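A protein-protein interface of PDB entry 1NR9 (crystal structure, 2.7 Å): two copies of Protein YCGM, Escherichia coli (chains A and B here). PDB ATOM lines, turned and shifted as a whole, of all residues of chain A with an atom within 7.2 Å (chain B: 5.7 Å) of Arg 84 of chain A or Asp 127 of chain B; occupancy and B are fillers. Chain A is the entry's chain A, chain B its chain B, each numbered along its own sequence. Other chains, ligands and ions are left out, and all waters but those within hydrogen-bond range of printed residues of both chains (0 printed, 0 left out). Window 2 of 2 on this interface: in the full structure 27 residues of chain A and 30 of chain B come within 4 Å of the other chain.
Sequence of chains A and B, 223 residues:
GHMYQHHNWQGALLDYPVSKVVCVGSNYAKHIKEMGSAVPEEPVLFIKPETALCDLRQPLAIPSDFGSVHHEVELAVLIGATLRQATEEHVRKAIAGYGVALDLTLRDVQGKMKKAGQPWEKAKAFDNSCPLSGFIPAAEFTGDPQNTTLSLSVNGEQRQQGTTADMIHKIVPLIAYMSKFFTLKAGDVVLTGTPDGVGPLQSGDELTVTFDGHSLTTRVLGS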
ATOM      1  N   LYS A  20       3.641  -5.801  19.830  1.00  0.00           N
ATOM      2  CA  LYS A  20       2.466  -5.094  19.349  1.00  0.00           C
ATOM      3  C   LYS A  20       2.240  -3.763  20.040  1.00  0.00           C
ATOM      4  O   LYS A  20       2.854  -3.447  21.057  1.00  0.00           O
ATOM      5  CB  LYS A  20       1.216  -5.956  19.516  1.00  0.00           C
ATOM      6  CG  LYS A  20       0.851  -6.258  20.949  1.00  0.00           C
ATOM      7  CD  LYS A  20      -0.536  -6.907  21.012  1.00  0.00           C
ATOM      8  CE  LYS A  20      -0.911  -7.302  22.429  1.00  0.00           C
ATOM      9  NZ  LYS A  20       0.035  -8.330  22.957  1.00  0.00           N
ATOM     10  N   ALA A  81       5.752  -5.697  32.214  1.00  0.00           N
ATOM     11  CA  ALA A  81       5.413  -7.043  32.671  1.00  0.00           C
ATOM     12  C   ALA A  81       4.065  -7.414  32.085  1.00  0.00           C
ATOM     13  O   ALA A  81       3.301  -6.542  31.674  1.00  0.00           O
ATOM     14  CB  ALA A  81       5.359  -7.085  34.183  1.00  0.00           C
ATOM     15  N   THR A  82       3.755  -8.701  32.063  1.00  0.00           N
ATOM     16  CA  THR A  82       2.512  -9.141  31.457  1.00  0.00           C
ATOM     17  C   THR A  82       1.219  -8.839  32.228  1.00  0.00           C
ATOM     18  O   THR A  82       1.136  -9.054  33.432  1.00  0.00           O
ATOM     19  CB  THR A  82       2.618 -10.631  31.095  1.00  0.00           C
ATOM     20  OG1 THR A  82       1.308 -11.193  30.992  1.00  0.00           O
ATOM     21  CG2 THR A  82       3.451 -11.374  32.118  1.00  0.00           C
ATOM     22  N   LEU A  83       0.217  -8.332  31.504  1.00  0.00           N
ATOM     23  CA  LEU A  83      -1.069  -7.956  32.074  1.00  0.00           C
ATOM     24  C   LEU A  83      -2.223  -8.654  31.356  1.00  0.00           C
ATOM     25  O   LEU A  83      -2.445  -8.433  30.167  1.00  0.00           O
ATOM     26  CB  LEU A  83      -1.269  -6.446  31.935  1.00  0.00           C
ATOM     27  CG  LEU A  83      -0.217  -5.454  32.452  1.00  0.00           C
ATOM     28  CD1 LEU A  83      -0.497  -4.086  31.869  1.00  0.00           C
ATOM     29  CD2 LEU A  83      -0.241  -5.395  33.973  1.00  0.00           C
ATOM     30  N   ARG A  84      -2.956  -9.497  32.079  1.00  0.00           N
ATOM     31  CA  ARG A  84      -4.100 -10.207  31.516  1.00  0.00           C
ATOM     32  C   ARG A  84      -5.245  -9.981  32.487  1.00  0.00           C
ATOM     33  O   ARG A  84      -5.094 -10.259  33.681  1.00  0.00           O
ATOM     34  CB  ARG A  84      -3.813 -11.705  31.393  1.00  0.00           C
ATOM     35  CG  ARG A  84      -5.027 -12.527  30.969  1.00  0.00           C
ATOM     36  CD  ARG A  84      -5.708 -11.899  29.753  1.00  0.00           C
ATOM     37  NE  ARG A  84      -6.892 -12.628  29.293  1.00  0.00           N
ATOM     38  CZ  ARG A  84      -7.680 -12.219  28.299  1.00  0.00           C
ATOM     39  NH1 ARG A  84      -7.411 -11.085  27.662  1.00  0.00           N
ATOM     40  NH2 ARG A  84      -8.732 -12.949  27.935  1.00  0.00           N
ATOM     41  N   GLN A  85      -6.371  -9.462  31.985  1.00  0.00           N
ATOM     42  CA  GLN A  85      -7.539  -9.185  32.831  1.00  0.00           C
ATOM     43  C   GLN A  85      -7.035  -8.559  34.139  1.00  0.00           C
ATOM     44  O   GLN A  85      -7.538  -8.853  35.215  1.00  0.00           O
ATOM     45  CB  GLN A  85      -8.285 -10.484  33.159  1.00  0.00           C
ATOM     46  CG  GLN A  85      -8.766 -11.301  31.967  1.00  0.00           C
ATOM     47  CD  GLN A  85     -10.013 -10.731  31.329  1.00  0.00           C
ATOM     48  OE1 GLN A  85     -11.024 -10.513  31.995  1.00  0.00           O
ATOM     49  NE2 GLN A  85      -9.951 -10.493  30.028  1.00  0.00           N
ATOM     50  N   ALA A  86      -6.039  -7.694  34.022  1.00  0.00           N
ATOM     51  CA  ALA A  86      -5.399  -7.057  35.164  1.00  0.00           C
ATOM     52  C   ALA A  86      -6.178  -6.011  35.950  1.00  0.00           C
ATOM     53  O   ALA A  86      -7.116  -5.392  35.451  1.00  0.00           O
ATOM     54  CB  ALA A  86      -4.082  -6.455  34.710  1.00  0.00           C
ATOM     55  N   THR A  87      -5.748  -5.819  37.193  1.00  0.00           N
ATOM     56  CA  THR A  87      -6.332  -4.829  38.088  1.00  0.00           C
ATOM     57  C   THR A  87      -5.440  -3.596  37.956  1.00  0.00           C
ATOM     58  O   THR A  87      -4.281  -3.699  37.542  1.00  0.00           O
ATOM     59  CB  THR A  87      -6.287  -5.280  39.568  1.00  0.00           C
ATOM     60  OG1 THR A  87      -4.953  -5.121  40.071  1.00  0.00           O
ATOM     61  CG2 THR A  87      -6.693  -6.736  39.705  1.00  0.00           C
ATOM     62  N   HIS A  90      -2.003  -3.755  39.292  1.00  0.00           N
ATOM     63  CA  HIS A  90      -1.088  -4.487  38.425  1.00  0.00           C
ATOM     64  C   HIS A  90      -0.577  -3.563  37.323  1.00  0.00           C
ATOM     65  O   HIS A  90       0.630  -3.472  37.087  1.00  0.00           O
ATOM     66  CB  HIS A  90      -1.807  -5.697  37.829  1.00  0.00           C
ATOM     67  CG  HIS A  90      -2.093  -6.778  38.826  1.00  0.00           C
ATOM     68  ND1 HIS A  90      -3.125  -7.681  38.675  1.00  0.00           N
ATOM     69  CD2 HIS A  90      -1.462  -7.119  39.976  1.00  0.00           C
ATOM     70  CE1 HIS A  90      -3.117  -8.529  39.686  1.00  0.00           C
ATOM     71  NE2 HIS A  90      -2.118  -8.211  40.490  1.00  0.00           N
ATOM     72  N   ALA A 176      -5.898  -1.204  31.862  1.00  0.00           N
ATOM     73  CA  ALA A 176      -6.591  -2.261  32.581  1.00  0.00           C
ATOM     74  C   ALA A 176      -7.705  -2.794  31.693  1.00  0.00           C
ATOM     75  O   ALA A 176      -7.873  -3.995  31.578  1.00  0.00           O
ATOM     76  CB  ALA A 176      -7.163  -1.725  33.884  1.00  0.00           C
ATOM     77  N   MET A 178      -7.939  -2.571  28.345  1.00  0.00           N
ATOM     78  CA  MET A 178      -7.331  -3.240  27.200  1.00  0.00           C
ATOM     79  C   MET A 178      -7.020  -4.693  27.510  1.00  0.00           C
ATOM     80  O   MET A 178      -7.372  -5.581  26.740  1.00  0.00           O
ATOM     81  CB  MET A 178      -6.037  -2.537  26.787  1.00  0.00           C
ATOM     82  CG  MET A 178      -6.257  -1.156  26.188  1.00  0.00           C
ATOM     83  SD  MET A 178      -4.629  -0.154  25.839  1.00  0.00           S
ATOM     84  CE  MET A 178      -5.322   0.927  24.377  1.00  0.00           C
ATOM     85  N   SER A 179      -6.358  -4.934  28.637  1.00  0.00           N
ATOM     86  CA  SER A 179      -5.982  -6.289  29.014  1.00  0.00           C
ATOM     87  C   SER A 179      -7.146  -7.262  29.004  1.00  0.00           C
ATOM     88  O   SER A 179      -6.938  -8.474  28.981  1.00  0.00           O
ATOM     89  CB  SER A 179      -5.307  -6.303  30.389  1.00  0.00           C
ATOM     90  OG  SER A 179      -6.168  -5.813  31.395  1.00  0.00           O
ATOM     91  N   LYS A 180      -8.369  -6.739  29.013  1.00  0.00           N
ATOM     92  CA  LYS A 180      -9.545  -7.602  28.998  1.00  0.00           C
ATOM     93  C   LYS A 180      -9.681  -8.401  27.703  1.00  0.00           C
ATOM     94  O   LYS A 180     -10.137  -9.543  27.721  1.00  0.00           O
ATOM     95  CB  LYS A 180     -10.812  -6.785  29.220  1.00  0.00           C
ATOM     96  CG  LYS A 180     -11.216  -6.640  30.674  1.00  0.00           C
ATOM     97  CD  LYS A 180     -12.537  -5.883  30.778  1.00  0.00           C
ATOM     98  CE  LYS A 180     -13.644  -6.580  29.980  1.00  0.00           C
ATOM     99  NZ  LYS A 180     -14.864  -5.732  29.768  1.00  0.00           N
ATOM    100  N   PHE A 181      -9.280  -7.809  26.583  1.00  0.00           N
ATOM    101  CA  PHE A 181      -9.379  -8.485  25.294  1.00  0.00           C
ATOM    102  C   PHE A 181      -8.044  -9.047  24.822  1.00  0.00           C
ATOM    103  O   PHE A 181      -7.995 -10.127  24.223  1.00  0.00           O
ATOM    104  CB  PHE A 181      -9.939  -7.529  24.253  1.00  0.00           C
ATOM    105  CG  PHE A 181     -11.152  -6.787  24.723  1.00  0.00           C
ATOM    106  CD1 PHE A 181     -11.032  -5.740  25.635  1.00  0.00           C
ATOM    107  CD2 PHE A 181     -12.423  -7.161  24.289  1.00  0.00           C
ATOM    108  CE1 PHE A 181     -12.155  -5.082  26.110  1.00  0.00           C
ATOM    109  CE2 PHE A 181     -13.551  -6.512  24.755  1.00  0.00           C
ATOM    110  CZ  PHE A 181     -13.421  -5.468  25.667  1.00  0.00           C
ATOM    111  N   PHE A 182      -6.961  -8.333  25.095  1.00  0.00           N
ATOM    112  CA  PHE A 182      -5.655  -8.801  24.675  1.00  0.00           C
ATOM    113  C   PHE A 182      -4.677  -8.739  25.824  1.00  0.00           C
ATOM    114  O   PHE A 182      -4.575  -7.714  26.502  1.00  0.00           O
ATOM    115  CB  PHE A 182      -5.115  -7.945  23.532  1.00  0.00           C
ATOM    116  CG  PHE A 182      -6.174  -7.203  22.768  1.00  0.00           C
ATOM    117  CD1 PHE A 182      -6.318  -5.831  22.919  1.00  0.00           C
ATOM    118  CD2 PHE A 182      -7.052  -7.882  21.915  1.00  0.00           C
ATOM    119  CE1 PHE A 182      -7.310  -5.159  22.238  1.00  0.00           C
ATOM    120  CE2 PHE A 182      -8.048  -7.215  21.231  1.00  0.00           C
ATOM    121  CZ  PHE A 182      -8.182  -5.859  21.389  1.00  0.00           C
ATOM    122  N   THR A 183      -3.950  -9.826  26.043  1.00  0.00           N
ATOM    123  CA  THR A 183      -2.970  -9.843  27.111  1.00  0.00           C
ATOM    124  C   THR A 183      -1.769  -9.021  26.658  1.00  0.00           C
ATOM    125  O   THR A 183      -1.238  -9.256  25.577  1.00  0.00           O
ATOM    126  CB  THR A 183      -2.510 -11.265  27.413  1.00  0.00           C
ATOM    127  OG1 THR A 183      -1.310 -11.215  28.185  1.00  0.00           O
ATOM    128  CG2 THR A 183      -2.235 -12.007  26.135  1.00  0.00           C
ATOM    129  N   LEU A 184      -1.354  -8.044  27.466  1.00  0.00           N
ATOM    130  CA  LEU A 184      -0.210  -7.206  27.116  1.00  0.00           C
ATOM    131  C   LEU A 184       1.046  -7.804  27.727  1.00  0.00           C
ATOM    132  O   LEU A 184       1.162  -7.913  28.952  1.00  0.00           O
ATOM    133  CB  LEU A 184      -0.384  -5.793  27.666  1.00  0.00           C
ATOM    134  CG  LEU A 184      -1.766  -5.153  27.557  1.00  0.00           C
ATOM    135  CD1 LEU A 184      -1.727  -3.791  28.229  1.00  0.00           C
ATOM    136  CD2 LEU A 184      -2.194  -5.021  26.095  1.00  0.00           C
ATOM    137  N   THR B  51      -0.222 -12.876  20.657  1.00  0.00           N
ATOM    138  CA  THR B  51      -0.982 -13.420  21.769  1.00  0.00           C
ATOM    139  C   THR B  51      -2.262 -14.176  21.381  1.00  0.00           C
ATOM    140  O   THR B  51      -2.976 -14.672  22.247  1.00  0.00           O
ATOM    141  CB  THR B  51      -1.350 -12.310  22.736  1.00  0.00           C
ATOM    142  OG1 THR B  51      -1.917 -11.222  22.002  1.00  0.00           O
ATOM    143  CG2 THR B  51      -0.127 -11.837  23.484  1.00  0.00           C
ATOM    144  N   ALA B  52      -2.563 -14.263  20.091  1.00  0.00           N
ATOM    145  CA  ALA B  52      -3.758 -14.974  19.663  1.00  0.00           C
ATOM    146  C   ALA B  52      -3.364 -16.381  19.243  1.00  0.00           C
ATOM    147  O   ALA B  52      -4.216 -17.281  19.099  1.00  0.00           O
ATOM    148  CB  ALA B  52      -4.395 -14.260  18.512  1.00  0.00           C
ATOM    149  N   ALA B  61      -9.120 -22.637  24.551  1.00  0.00           N
ATOM    150  CA  ALA B  61      -9.738 -21.790  25.554  1.00  0.00           C
ATOM    151  C   ALA B  61     -10.441 -20.638  24.850  1.00  0.00           C
ATOM    152  O   ALA B  61      -9.842 -19.927  24.040  1.00  0.00           O
ATOM    153  CB  ALA B  61      -8.692 -21.256  26.500  1.00  0.00           C
ATOM    154  N   PRO B  63     -13.395 -17.233  25.301  1.00  0.00           N
ATOM    155  CA  PRO B  63     -13.995 -16.328  26.288  1.00  0.00           C
ATOM    156  C   PRO B  63     -15.446 -16.766  26.490  1.00  0.00           C
ATOM    157  O   PRO B  63     -16.096 -17.249  25.556  1.00  0.00           O
ATOM    158  CB  PRO B  63     -13.902 -14.951  25.613  1.00  0.00           C
ATOM    159  CG  PRO B  63     -12.883 -15.135  24.496  1.00  0.00           C
ATOM    160  CD  PRO B  63     -13.163 -16.536  24.026  1.00  0.00           C
ATOM    161  N   ALA B 125      -8.949 -10.453  17.413  1.00  0.00           N
ATOM    162  CA  ALA B 125      -7.611 -10.484  17.975  1.00  0.00           C
ATOM    163  C   ALA B 125      -7.515 -10.835  19.447  1.00  0.00           C
ATOM    164  O   ALA B 125      -6.449 -10.678  20.041  1.00  0.00           O
ATOM    165  CB  ALA B 125      -6.915  -9.135  17.720  1.00  0.00           C
ATOM    166  N   PHE B 126      -8.600 -11.301  20.054  1.00  0.00           N
ATOM    167  CA  PHE B 126      -8.531 -11.647  21.477  1.00  0.00           C
ATOM    168  C   PHE B 126      -7.529 -12.779  21.725  1.00  0.00           C
ATOM    169  O   PHE B 126      -6.980 -13.352  20.782  1.00  0.00           O
ATOM    170  CB  PHE B 126      -9.907 -12.045  22.004  1.00  0.00           C
ATOM    171  CG  PHE B 126     -10.531 -13.198  21.281  1.00  0.00           C
ATOM    172  CD1 PHE B 126     -11.297 -12.986  20.141  1.00  0.00           C
ATOM    173  CD2 PHE B 126     -10.390 -14.496  21.767  1.00  0.00           C
ATOM    174  CE1 PHE B 126     -11.913 -14.049  19.496  1.00  0.00           C
ATOM    175  CE2 PHE B 126     -10.998 -15.561  21.131  1.00  0.00           C
ATOM    176  CZ  PHE B 126     -11.765 -15.340  19.994  1.00  0.00           C
ATOM    177  N   ASP B 127      -7.284 -13.108  22.985  1.00  0.00           N
ATOM    178  CA  ASP B 127      -6.319 -14.153  23.296  1.00  0.00           C
ATOM    179  C   ASP B 127      -6.697 -15.549  22.846  1.00  0.00           C
ATOM    180  O   ASP B 127      -7.817 -16.019  23.086  1.00  0.00           O
ATOM    181  CB  ASP B 127      -6.045 -14.193  24.791  1.00  0.00           C
ATOM    182  CG  ASP B 127      -5.220 -13.026  25.262  1.00  0.00           C
ATOM    183  OD1 ASP B 127      -4.986 -12.088  24.462  1.00  0.00           O
ATOM    184  OD2 ASP B 127      -4.813 -13.058  26.446  1.00  0.00           O
ATOM    185  N   ASN B 128      -5.742 -16.215  22.205  1.00  0.00           N
ATOM    186  CA  ASN B 128      -5.930 -17.582  21.735  1.00  0.00           C
ATOM    187  C   ASN B 128      -7.019 -17.651  20.687  1.00  0.00           C
ATOM    188  O   ASN B 128      -7.631 -18.693  20.479  1.00  0.00           O
ATOM    189  CB  ASN B 128      -6.267 -18.504  22.912  1.00  0.00           C
ATOM    190  CG  ASN B 128      -5.275 -18.365  24.061  1.00  0.00           C
ATOM    191  OD1 ASN B 128      -4.070 -18.592  23.908  1.00  0.00           O
ATOM    192  ND2 ASN B 128      -5.786 -17.982  25.222  1.00  0.00           N
ATOM    193  N   SER B 129      -7.238 -16.524  20.020  1.00  0.00           N
ATOM    194  CA  SER B 129      -8.238 -16.421  18.969  1.00  0.00           C
ATOM    195  C   SER B 129      -7.707 -17.074  17.690  1.00  0.00           C
ATOM    196  O   SER B 129      -8.308 -16.940  16.615  1.00  0.00           O
ATOM    197  CB  SER B 129      -8.524 -14.953  18.673  1.00  0.00           C
ATOM    198  OG  SER B 129      -7.356 -14.347  18.123  1.00  0.00           O
ATOM    199  N   CYS B 130      -6.581 -17.773  17.794  1.00  0.00           N
ATOM    200  CA  CYS B 130      -6.028 -18.394  16.605  1.00  0.00           C
ATOM    201  C   CYS B 130      -5.323 -19.726  16.842  1.00  0.00           C
ATOM    202  O   CYS B 130      -4.089 -19.789  16.881  1.00  0.00           O
ATOM    203  CB  CYS B 130      -5.075 -17.410  15.926  1.00  0.00           C
ATOM    204  SG  CYS B 130      -4.583 -17.852  14.252  1.00  0.00           S
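NZ of Lys 20 of chain A sits at hydrogen-bond distance from O of Thr 183 of chain A, 3.1 Å away.
The guanidinium group of Arg 84 of chain A sits close to the side-chain amide nitrogen of Gln 85 of chain A, at 3.4 Å.
NH1 of Arg 84 of chain A is in hydrogen-bond range of O of Ser 179 of chain A (3.0 Å).
The guanidinium group of Arg 84 of chain A is in hydrogen-bond range of the backbone carbonyl oxygen of Lys 180 of chain A.
The backbone carbonyl oxygen (O) of Thr 51 of chain B sits at hydrogen-bond distance from the backbone NH (N) of Asn 128 of chain B (3.2 Å).
The backbone carbonyl oxygen (O) of Phe 126 of chain B is in hydrogen-bond range of the side-chain hydroxyl (OG) of Ser 129 of chain B, 2.9 Å away.
Of the printed residues of chain B, Arg 84 of chain A touches Asp 127.
Of the printed residues of chain B, Phe 181 of chain A touches Phe 126 (3.2 Å) and Asp 127 (3.3 Å).
Printed residues of chain A within 4 Å of Thr 51 of chain B: Lys 20 and Thr 183.
Printed residues of chain B within 4 Å of Phe 182 of chain A: Ala 125 (3.4 Å) and Asp 127 (3.4 Å).
Leu 83 of chain A touches none of the printed residues of chain B.
Ala 81 of chain A touches none of the printed residues of chain B.
No position is printed for both chains.
Of the 10 printed residues of chain B, 4 touch a printed residue of chain A.
Hydrophobic or aromatic side chains of chain B within 4 Å of the printed part of chain A: Phe 126.
Printed residues of chain A that touch a printed residue of chain B: Lys 20, Arg 84, Phe 181, Phe 182 and Thr 183.
Among the printed residues, 8 pairs touch across the chains.
Among the printed residues, pairs that only touch across the chains: Lys 20 of chain A with Thr 51 of chain B, Phe 181 of chain A with Phe 126 of chain B, Phe 182 of chain A with Ala 125 of chain B, Phe 182 of chain A with Asp 127 of chain B and Thr 183 of chain A with Thr 51 of chain B.
The guanidinium group (NH1) of Arg 84 of chain A is in salt-bridge range of the side-chain carboxylate (OD2) of Asp 127 of chain B (3.5 Å).
The backbone carbonyl oxygen (O) of Phe 181 of chain A lies within hydrogen-bond range of the backbone NH (N) of Asp 127 of chain B (3.3 Å).
N of Thr 183 of chain A lies within hydrogen-bond range of OD1 of Asp 127 of chain B (2.9 Å).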
